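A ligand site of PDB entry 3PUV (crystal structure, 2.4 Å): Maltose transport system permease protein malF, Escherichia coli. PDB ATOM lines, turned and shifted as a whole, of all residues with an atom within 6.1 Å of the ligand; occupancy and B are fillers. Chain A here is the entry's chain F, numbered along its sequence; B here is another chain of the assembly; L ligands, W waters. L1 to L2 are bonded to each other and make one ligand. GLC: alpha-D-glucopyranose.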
ATOM      1  N   THR A 291     -16.025 -21.229 -31.964  1.00  0.00           N
ATOM      2  CA  THR A 291     -16.724 -22.153 -31.068  1.00  0.00           C
ATOM      3  C   THR A 291     -15.816 -23.299 -30.633  1.00  0.00           C
ATOM      4  O   THR A 291     -15.635 -23.542 -29.443  1.00  0.00           O
ATOM      5  CB  THR A 291     -18.011 -22.737 -31.716  1.00  0.00           C
ATOM      6  OG1 THR A 291     -18.914 -21.679 -32.039  1.00  0.00           O
ATOM      7  CG2 THR A 291     -18.698 -23.705 -30.753  1.00  0.00           C
ATOM      8  N   VAL A 292     -15.216 -23.986 -31.616  1.00  0.00           N
ATOM      9  CA  VAL A 292     -14.361 -25.137 -31.360  1.00  0.00           C
ATOM     10  C   VAL A 292     -13.173 -24.749 -30.476  1.00  0.00           C
ATOM     11  O   VAL A 292     -12.894 -25.401 -29.472  1.00  0.00           O
ATOM     12  CB  VAL A 292     -13.890 -25.826 -32.670  1.00  0.00           C
ATOM     13  CG1 VAL A 292     -12.881 -26.941 -32.397  1.00  0.00           C
ATOM     14  CG2 VAL A 292     -15.084 -26.383 -33.436  1.00  0.00           C
ATOM     15  N   THR A 295     -14.580 -23.788 -26.878  1.00  0.00           N
ATOM     16  CA  THR A 295     -15.115 -24.957 -26.157  1.00  0.00           C
ATOM     17  C   THR A 295     -13.998 -25.910 -25.743  1.00  0.00           C
ATOM     18  O   THR A 295     -14.011 -26.453 -24.634  1.00  0.00           O
ATOM     19  CB  THR A 295     -16.226 -25.704 -26.938  1.00  0.00           C
ATOM     20  OG1 THR A 295     -15.781 -25.991 -28.265  1.00  0.00           O
ATOM     21  CG2 THR A 295     -17.489 -24.853 -27.007  1.00  0.00           C
ATOM     22  N   TYR A 325     -25.169 -29.292 -20.143  1.00  0.00           N
ATOM     23  CA  TYR A 325     -25.271 -30.345 -21.149  1.00  0.00           C
ATOM     24  C   TYR A 325     -26.267 -31.421 -20.699  1.00  0.00           C
ATOM     25  O   TYR A 325     -26.725 -32.231 -21.515  1.00  0.00           O
ATOM     26  CB  TYR A 325     -23.880 -30.948 -21.369  1.00  0.00           C
ATOM     27  CG  TYR A 325     -23.685 -31.796 -22.613  1.00  0.00           C
ATOM     28  CD1 TYR A 325     -24.367 -31.511 -23.804  1.00  0.00           C
ATOM     29  CD2 TYR A 325     -22.772 -32.849 -22.616  1.00  0.00           C
ATOM     30  CE1 TYR A 325     -24.156 -32.284 -24.943  1.00  0.00           C
ATOM     31  CE2 TYR A 325     -22.565 -33.620 -23.741  1.00  0.00           C
ATOM     32  CZ  TYR A 325     -23.250 -33.341 -24.902  1.00  0.00           C
ATOM     33  OH  TYR A 325     -23.021 -34.114 -26.019  1.00  0.00           O
ATOM     34  N   SER A 329     -31.140 -28.643 -24.508  1.00  0.00           N
ATOM     35  CA  SER A 329     -30.691 -27.311 -24.913  1.00  0.00           C
ATOM     36  C   SER A 329     -31.793 -26.387 -25.422  1.00  0.00           C
ATOM     37  O   SER A 329     -31.658 -25.162 -25.356  1.00  0.00           O
ATOM     38  CB  SER A 329     -29.594 -27.435 -25.977  1.00  0.00           C
ATOM     39  OG  SER A 329     -30.121 -27.924 -27.196  1.00  0.00           O
ATOM     40  N   ILE A 333     -31.742 -22.325 -24.848  1.00  0.00           N
ATOM     41  CA  ILE A 333     -31.557 -21.369 -25.930  1.00  0.00           C
ATOM     42  C   ILE A 333     -32.603 -20.254 -25.872  1.00  0.00           C
ATOM     43  O   ILE A 333     -32.282 -19.083 -26.065  1.00  0.00           O
ATOM     44  CB  ILE A 333     -31.534 -22.057 -27.313  1.00  0.00           C
ATOM     45  CG1 ILE A 333     -30.371 -23.066 -27.383  1.00  0.00           C
ATOM     46  CG2 ILE A 333     -31.404 -21.036 -28.435  1.00  0.00           C
ATOM     47  CD1 ILE A 333     -30.421 -24.024 -28.559  1.00  0.00           C
ATOM     48  N   ASN A 376     -23.172 -20.539 -27.404  1.00  0.00           N
ATOM     49  CA  ASN A 376     -22.667 -21.782 -27.999  1.00  0.00           C
ATOM     50  C   ASN A 376     -21.526 -22.405 -27.203  1.00  0.00           C
ATOM     51  O   ASN A 376     -21.409 -23.633 -27.112  1.00  0.00           O
ATOM     52  CB  ASN A 376     -22.256 -21.554 -29.453  1.00  0.00           C
ATOM     53  CG  ASN A 376     -22.396 -22.800 -30.295  1.00  0.00           C
ATOM     54  OD1 ASN A 376     -23.199 -23.684 -30.001  1.00  0.00           O
ATOM     55  ND2 ASN A 376     -21.632 -22.858 -31.375  1.00  0.00           N
ATOM     56  N   THR A 377     -20.668 -21.553 -26.639  1.00  0.00           N
ATOM     57  CA  THR A 377     -19.608 -21.983 -25.736  1.00  0.00           C
ATOM     58  C   THR A 377     -20.213 -22.555 -24.454  1.00  0.00           C
ATOM     59  O   THR A 377     -19.703 -23.537 -23.910  1.00  0.00           O
ATOM     60  CB  THR A 377     -18.665 -20.818 -25.391  1.00  0.00           C
ATOM     61  OG1 THR A 377     -18.158 -20.246 -26.608  1.00  0.00           O
ATOM     62  CG2 THR A 377     -17.484 -21.290 -24.544  1.00  0.00           C
ATOM     63  N   LEU A 379     -23.159 -23.950 -24.321  1.00  0.00           N
ATOM     64  CA  LEU A 379     -23.747 -25.221 -24.741  1.00  0.00           C
ATOM     65  C   LEU A 379     -22.681 -26.301 -24.930  1.00  0.00           C
ATOM     66  O   LEU A 379     -22.913 -27.473 -24.598  1.00  0.00           O
ATOM     67  CB  LEU A 379     -24.532 -25.058 -26.042  1.00  0.00           C
ATOM     68  CG  LEU A 379     -25.839 -24.247 -26.072  1.00  0.00           C
ATOM     69  CD1 LEU A 379     -26.359 -24.141 -27.505  1.00  0.00           C
ATOM     70  CD2 LEU A 379     -26.906 -24.829 -25.148  1.00  0.00           C
ATOM     71  N   GLY A 380     -21.513 -25.901 -25.438  1.00  0.00           N
ATOM     72  CA  GLY A 380     -20.513 -26.838 -25.931  1.00  0.00           C
ATOM     73  C   GLY A 380     -19.311 -27.189 -25.079  1.00  0.00           C
ATOM     74  O   GLY A 380     -18.586 -28.132 -25.392  1.00  0.00           O
ATOM     75  N   TYR A 381     -19.070 -26.431 -24.000  1.00  0.00           N
ATOM     76  CA  TYR A 381     -17.896 -26.710 -23.166  1.00  0.00           C
ATOM     77  C   TYR A 381     -17.943 -28.053 -22.397  1.00  0.00           C
ATOM     78  O   TYR A 381     -16.899 -28.702 -22.271  1.00  0.00           O
ATOM     79  CB  TYR A 381     -17.520 -25.530 -22.243  1.00  0.00           C
ATOM     80  CG  TYR A 381     -18.263 -25.449 -20.939  1.00  0.00           C
ATOM     81  CD1 TYR A 381     -17.880 -26.229 -19.840  1.00  0.00           C
ATOM     82  CD2 TYR A 381     -19.342 -24.592 -20.785  1.00  0.00           C
ATOM     83  CE1 TYR A 381     -18.565 -26.168 -18.642  1.00  0.00           C
ATOM     84  CE2 TYR A 381     -20.037 -24.516 -19.578  1.00  0.00           C
ATOM     85  CZ  TYR A 381     -19.639 -25.309 -18.509  1.00  0.00           C
ATOM     86  OH  TYR A 381     -20.325 -25.243 -17.320  1.00  0.00           O
ATOM     87  N   TYR A 383     -19.116 -30.934 -23.289  1.00  0.00           N
ATOM     88  CA  TYR A 383     -18.741 -31.996 -24.219  1.00  0.00           C
ATOM     89  C   TYR A 383     -17.221 -32.178 -24.245  1.00  0.00           C
ATOM     90  O   TYR A 383     -16.721 -33.277 -24.032  1.00  0.00           O
ATOM     91  CB  TYR A 383     -19.274 -31.683 -25.623  1.00  0.00           C
ATOM     92  CG  TYR A 383     -18.813 -32.634 -26.706  1.00  0.00           C
ATOM     93  CD1 TYR A 383     -19.303 -33.943 -26.772  1.00  0.00           C
ATOM     94  CD2 TYR A 383     -17.905 -32.222 -27.681  1.00  0.00           C
ATOM     95  CE1 TYR A 383     -18.895 -34.819 -27.767  1.00  0.00           C
ATOM     96  CE2 TYR A 383     -17.485 -33.097 -28.688  1.00  0.00           C
ATOM     97  CZ  TYR A 383     -17.989 -34.393 -28.723  1.00  0.00           C
ATOM     98  OH  TYR A 383     -17.569 -35.252 -29.710  1.00  0.00           O
ATOM     99  N   MET A 384     -16.512 -31.078 -24.487  1.00  0.00           N
ATOM    100  CA  MET A 384     -15.052 -31.083 -24.564  1.00  0.00           C
ATOM    101  C   MET A 384     -14.416 -31.371 -23.213  1.00  0.00           C
ATOM    102  O   MET A 384     -13.379 -32.046 -23.145  1.00  0.00           O
ATOM    103  CB  MET A 384     -14.542 -29.769 -25.141  1.00  0.00           C
ATOM    104  CG  MET A 384     -14.835 -29.606 -26.622  1.00  0.00           C
ATOM    105  SD  MET A 384     -14.068 -30.919 -27.614  1.00  0.00           S
ATOM    106  CE  MET A 384     -14.731 -30.506 -29.237  1.00  0.00           C
ATOM    107  N   LEU A 429     -11.742 -35.061 -33.089  1.00  0.00           N
ATOM    108  CA  LEU A 429     -12.912 -34.550 -32.383  1.00  0.00           C
ATOM    109  C   LEU A 429     -13.130 -33.068 -32.662  1.00  0.00           C
ATOM    110  O   LEU A 429     -14.274 -32.599 -32.702  1.00  0.00           O
ATOM    111  CB  LEU A 429     -12.799 -34.816 -30.883  1.00  0.00           C
ATOM    112  CG  LEU A 429     -12.849 -36.301 -30.514  1.00  0.00           C
ATOM    113  CD1 LEU A 429     -12.269 -36.566 -29.134  1.00  0.00           C
ATOM    114  CD2 LEU A 429     -14.268 -36.860 -30.641  1.00  0.00           C
ATOM    115  N   ALA A 432     -14.534 -32.760 -36.179  1.00  0.00           N
ATOM    116  CA  ALA A 432     -15.939 -33.155 -36.121  1.00  0.00           C
ATOM    117  C   ALA A 432     -16.784 -32.038 -35.527  1.00  0.00           C
ATOM    118  O   ALA A 432     -17.853 -31.711 -36.053  1.00  0.00           O
ATOM    119  CB  ALA A 432     -16.093 -34.427 -35.329  1.00  0.00           C
ATOM    120  N   SER A 433     -16.300 -31.448 -34.444  1.00  0.00           N
ATOM    121  CA  SER A 433     -16.965 -30.315 -33.790  1.00  0.00           C
ATOM    122  C   SER A 433     -17.062 -29.109 -34.718  1.00  0.00           C
ATOM    123  O   SER A 433     -17.974 -28.287 -34.574  1.00  0.00           O
ATOM    124  CB  SER A 433     -16.241 -29.941 -32.501  1.00  0.00           C
ATOM    125  OG  SER A 433     -16.976 -28.985 -31.751  1.00  0.00           O
ATOM    126  N   PHE A 434     -16.123 -29.001 -35.649  1.00  0.00           N
ATOM    127  CA  PHE A 434     -16.174 -27.951 -36.672  1.00  0.00           C
ATOM    128  C   PHE A 434     -17.292 -28.196 -37.668  1.00  0.00           C
ATOM    129  O   PHE A 434     -18.046 -27.284 -38.000  1.00  0.00           O
ATOM    130  CB  PHE A 434     -14.827 -27.824 -37.404  1.00  0.00           C
ATOM    131  CG  PHE A 434     -14.853 -26.850 -38.548  1.00  0.00           C
ATOM    132  CD1 PHE A 434     -15.065 -27.281 -39.845  1.00  0.00           C
ATOM    133  CD2 PHE A 434     -14.674 -25.485 -38.313  1.00  0.00           C
ATOM    134  CE1 PHE A 434     -15.098 -26.384 -40.915  1.00  0.00           C
ATOM    135  CE2 PHE A 434     -14.695 -24.574 -39.366  1.00  0.00           C
ATOM    136  CZ  PHE A 434     -14.918 -25.023 -40.671  1.00  0.00           C
ATOM    137  N   PHE A 436     -19.969 -30.117 -37.255  1.00  0.00           N
ATOM    138  CA  PHE A 436     -21.250 -30.070 -36.552  1.00  0.00           C
ATOM    139  C   PHE A 436     -21.701 -28.625 -36.377  1.00  0.00           C
ATOM    140  O   PHE A 436     -22.851 -28.295 -36.657  1.00  0.00           O
ATOM    141  CB  PHE A 436     -21.159 -30.775 -35.197  1.00  0.00           C
ATOM    142  CG  PHE A 436     -22.423 -30.700 -34.379  1.00  0.00           C
ATOM    143  CD1 PHE A 436     -22.583 -29.685 -33.426  1.00  0.00           C
ATOM    144  CD2 PHE A 436     -23.442 -31.630 -34.541  1.00  0.00           C
ATOM    145  CE1 PHE A 436     -23.754 -29.607 -32.660  1.00  0.00           C
ATOM    146  CE2 PHE A 436     -24.616 -31.559 -33.790  1.00  0.00           C
ATOM    147  CZ  PHE A 436     -24.777 -30.545 -32.836  1.00  0.00           C
ATOM    148  N   ASN A 437     -20.792 -27.761 -35.913  1.00  0.00           N
ATOM    149  CA  ASN A 437     -21.107 -26.354 -35.713  1.00  0.00           C
ATOM    150  C   ASN A 437     -21.209 -25.554 -37.008  1.00  0.00           C
ATOM    151  O   ASN A 437     -21.785 -24.460 -37.025  1.00  0.00           O
ATOM    152  CB  ASN A 437     -20.110 -25.702 -34.746  1.00  0.00           C
ATOM    153  CG  ASN A 437     -20.408 -26.040 -33.290  1.00  0.00           C
ATOM    154  OD1 ASN A 437     -19.581 -26.655 -32.598  1.00  0.00           O
ATOM    155  ND2 ASN A 437     -21.588 -25.660 -32.820  1.00  0.00           N
ATOM    156  N   ASN A 440     -24.974 -25.912 -37.622  1.00  0.00           N
ATOM    157  CA  ASN A 440     -25.755 -25.699 -36.405  1.00  0.00           C
ATOM    158  C   ASN A 440     -27.023 -24.864 -36.617  1.00  0.00           C
ATOM    159  O   ASN A 440     -27.187 -23.787 -36.037  1.00  0.00           O
ATOM    160  CB  ASN A 440     -24.882 -25.083 -35.320  1.00  0.00           C
ATOM    161  CG  ASN A 440     -25.307 -25.488 -33.910  1.00  0.00           C
ATOM    162  OD1 ASN A 440     -24.496 -25.497 -32.984  1.00  0.00           O
ATOM    163  ND2 ASN A 440     -26.590 -25.824 -33.754  1.00  0.00           N
ATOM    164  N   LEU A 443     -29.493 -23.559 -33.355  1.00  0.00           N
ATOM    165  CA  LEU A 443     -29.049 -22.464 -32.505  1.00  0.00           C
ATOM    166  C   LEU A 443     -29.434 -21.095 -33.063  1.00  0.00           C
ATOM    167  O   LEU A 443     -29.983 -20.256 -32.346  1.00  0.00           O
ATOM    168  CB  LEU A 443     -27.546 -22.526 -32.242  1.00  0.00           C
ATOM    169  CG  LEU A 443     -26.943 -21.348 -31.476  1.00  0.00           C
ATOM    170  CD1 LEU A 443     -27.461 -21.275 -30.039  1.00  0.00           C
ATOM    171  CD2 LEU A 443     -25.438 -21.403 -31.504  1.00  0.00           C
ATOM    172  N   LEU B 172     -17.316 -41.506 -34.292  1.00  0.00           N
ATOM    173  CA  LEU B 172     -16.489 -40.651 -33.441  1.00  0.00           C
ATOM    174  C   LEU B 172     -15.983 -41.370 -32.198  1.00  0.00           C
ATOM    175  O   LEU B 172     -14.836 -41.173 -31.793  1.00  0.00           O
ATOM    176  CB  LEU B 172     -17.237 -39.381 -33.060  1.00  0.00           C
ATOM    177  CG  LEU B 172     -17.056 -38.195 -34.000  1.00  0.00           C
ATOM    178  CD1 LEU B 172     -17.931 -37.052 -33.559  1.00  0.00           C
ATOM    179  CD2 LEU B 172     -15.587 -37.776 -34.040  1.00  0.00           C
ATOM    180  N   LEU B 221     -21.139 -39.837 -22.837  1.00  0.00           N
ATOM    181  CA  LEU B 221     -21.510 -39.099 -24.037  1.00  0.00           C
ATOM    182  C   LEU B 221     -22.688 -39.709 -24.787  1.00  0.00           C
ATOM    183  O   LEU B 221     -23.481 -38.987 -25.383  1.00  0.00           O
ATOM    184  CB  LEU B 221     -20.313 -38.925 -24.969  1.00  0.00           C
ATOM    185  CG  LEU B 221     -19.245 -37.938 -24.489  1.00  0.00           C
ATOM    186  CD1 LEU B 221     -18.042 -37.974 -25.405  1.00  0.00           C
ATOM    187  CD2 LEU B 221     -19.782 -36.526 -24.369  1.00  0.00           C
ATOM    188  N   ALA B 225     -26.606 -38.221 -25.092  1.00  0.00           N
ATOM    189  CA  ALA B 225     -27.115 -38.216 -26.454  1.00  0.00           C
ATOM    190  C   ALA B 225     -28.509 -38.853 -26.533  1.00  0.00           C
ATOM    191  O   ALA B 225     -29.422 -38.287 -27.130  1.00  0.00           O
ATOM    192  CB  ALA B 225     -26.140 -38.937 -27.375  1.00  0.00           C
HETATM  193  C1  GLC L   1     -21.408 -34.272 -30.645  1.00  0.00           C
HETATM  194  C2  GLC L   1     -22.316 -34.229 -29.413  1.00  0.00           C
HETATM  195  C3  GLC L   1     -23.099 -32.919 -29.357  1.00  0.00           C
HETATM  196  C4  GLC L   1     -22.137 -31.724 -29.393  1.00  0.00           C
HETATM  197  C5  GLC L   1     -21.281 -31.826 -30.661  1.00  0.00           C
HETATM  198  C6  GLC L   1     -20.237 -30.707 -30.698  1.00  0.00           C
HETATM  199  O1  GLC L   1     -22.165 -34.450 -31.841  1.00  0.00           O
HETATM  200  O2  GLC L   1     -23.228 -35.331 -29.425  1.00  0.00           O
HETATM  201  O3  GLC L   1     -23.913 -32.873 -28.178  1.00  0.00           O
HETATM  202  O4  GLC L   1     -22.878 -30.506 -29.433  1.00  0.00           O
HETATM  203  O5  GLC L   1     -20.604 -33.090 -30.740  1.00  0.00           O
HETATM  204  O6  GLC L   1     -19.292 -31.005 -31.726  1.00  0.00           O
HETATM  205  C1  GLC L   2     -22.837 -29.720 -28.232  1.00  0.00           C
HETATM  206  C2  GLC L   2     -24.255 -29.231 -27.898  1.00  0.00           C
HETATM  207  C3  GLC L   2     -24.758 -28.218 -28.934  1.00  0.00           C
HETATM  208  C4  GLC L   2     -23.740 -27.110 -29.199  1.00  0.00           C
HETATM  209  C5  GLC L   2     -22.332 -27.677 -29.437  1.00  0.00           C
HETATM  210  C6  GLC L   2     -21.301 -26.562 -29.508  1.00  0.00           C
HETATM  211  O2  GLC L   2     -25.150 -30.348 -27.840  1.00  0.00           O
HETATM  212  O3  GLC L   2     -25.975 -27.625 -28.452  1.00  0.00           O
HETATM  213  O4  GLC L   2     -24.157 -26.356 -30.342  1.00  0.00           O
HETATM  214  O5  GLC L   2     -21.959 -28.595 -28.397  1.00  0.00           O
HETATM  215  O6  GLC L   2     -20.093 -27.068 -30.080  1.00  0.00           O
HETATM  216  O   HOH W   1     -26.345 -34.992 -27.042  1.00  0.00           O
HETATM  217  O   HOH W   2     -26.951 -26.076 -31.178  1.00  0.00           O
HETATM  218  O   HOH W   3     -18.690 -28.976 -27.870  1.00  0.00           O
HETATM  219  O   HOH W   4     -20.134 -34.664 -34.446  1.00  0.00           O
HETATM  220  O   HOH W   5     -22.629 -37.050 -27.429  1.00  0.00           O
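OD1 of Asn 437 is in hydrogen-bond range of O6 of GLC L2 (2.6 Å).
OH of Tyr 325 is in hydrogen-bond range of O3 of GLC L1 (2.6 Å).
An oxygen (O4) of GLC L2 lies within hydrogen-bond range of the side-chain amide oxygen (OD1) of Asn 440, at 2.8 Å.
An oxygen (O4) of GLC L2 is in hydrogen-bond range of the side-chain amide oxygen (OD1) of Asn 376.
O6 of GLC L1 lies within hydrogen-bond range of OG of Ser 433.
Water W5 lies within hydrogen-bond range of an oxygen (O2) of GLC L1 (2.7 Å), the backbone carbonyl oxygen (O) of Leu 221 of chain B (2.9 Å) and the side-chain hydroxyl (OH) of Tyr 325 (3.3 Å).
Water W2 bridges the side-chain amide nitrogen of Asn 440 (2.6 Å) and an oxygen (O4) of GLC L2 (2.9 Å).
Water W3 bridges O of Gly 380 (2.6 Å) and O6 of GLC L2 (3.2 Å).
Merely in contact with the ligand: Gly 380, Phe 436, Tyr 383, Leu 379 and Thr 291.
Of the 24 residues printed, 10 come within 4 Å of the ligand.
ND2 of Asn 437 is in hydrogen-bond range of OD1 of Asn 440, 2.9 Å away.
ND2 of Asn 437 lies close to ND2 of Asn 376.
The backbone carbonyl oxygen (O) of Ser 433 sits close to the side-chain amide oxygen (OD1) of Asn 437, at 3.0 Å.
The side-chain amide nitrogen (ND2) of Asn 376 sits at hydrogen-bond distance from the side-chain hydroxyl (OG1) of Thr 291 (3.0 Å).
The backbone carbonyl oxygen (O) of Thr 291 sits at hydrogen-bond distance from the side-chain hydroxyl (OG1) of Thr 295 (2.7 Å).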
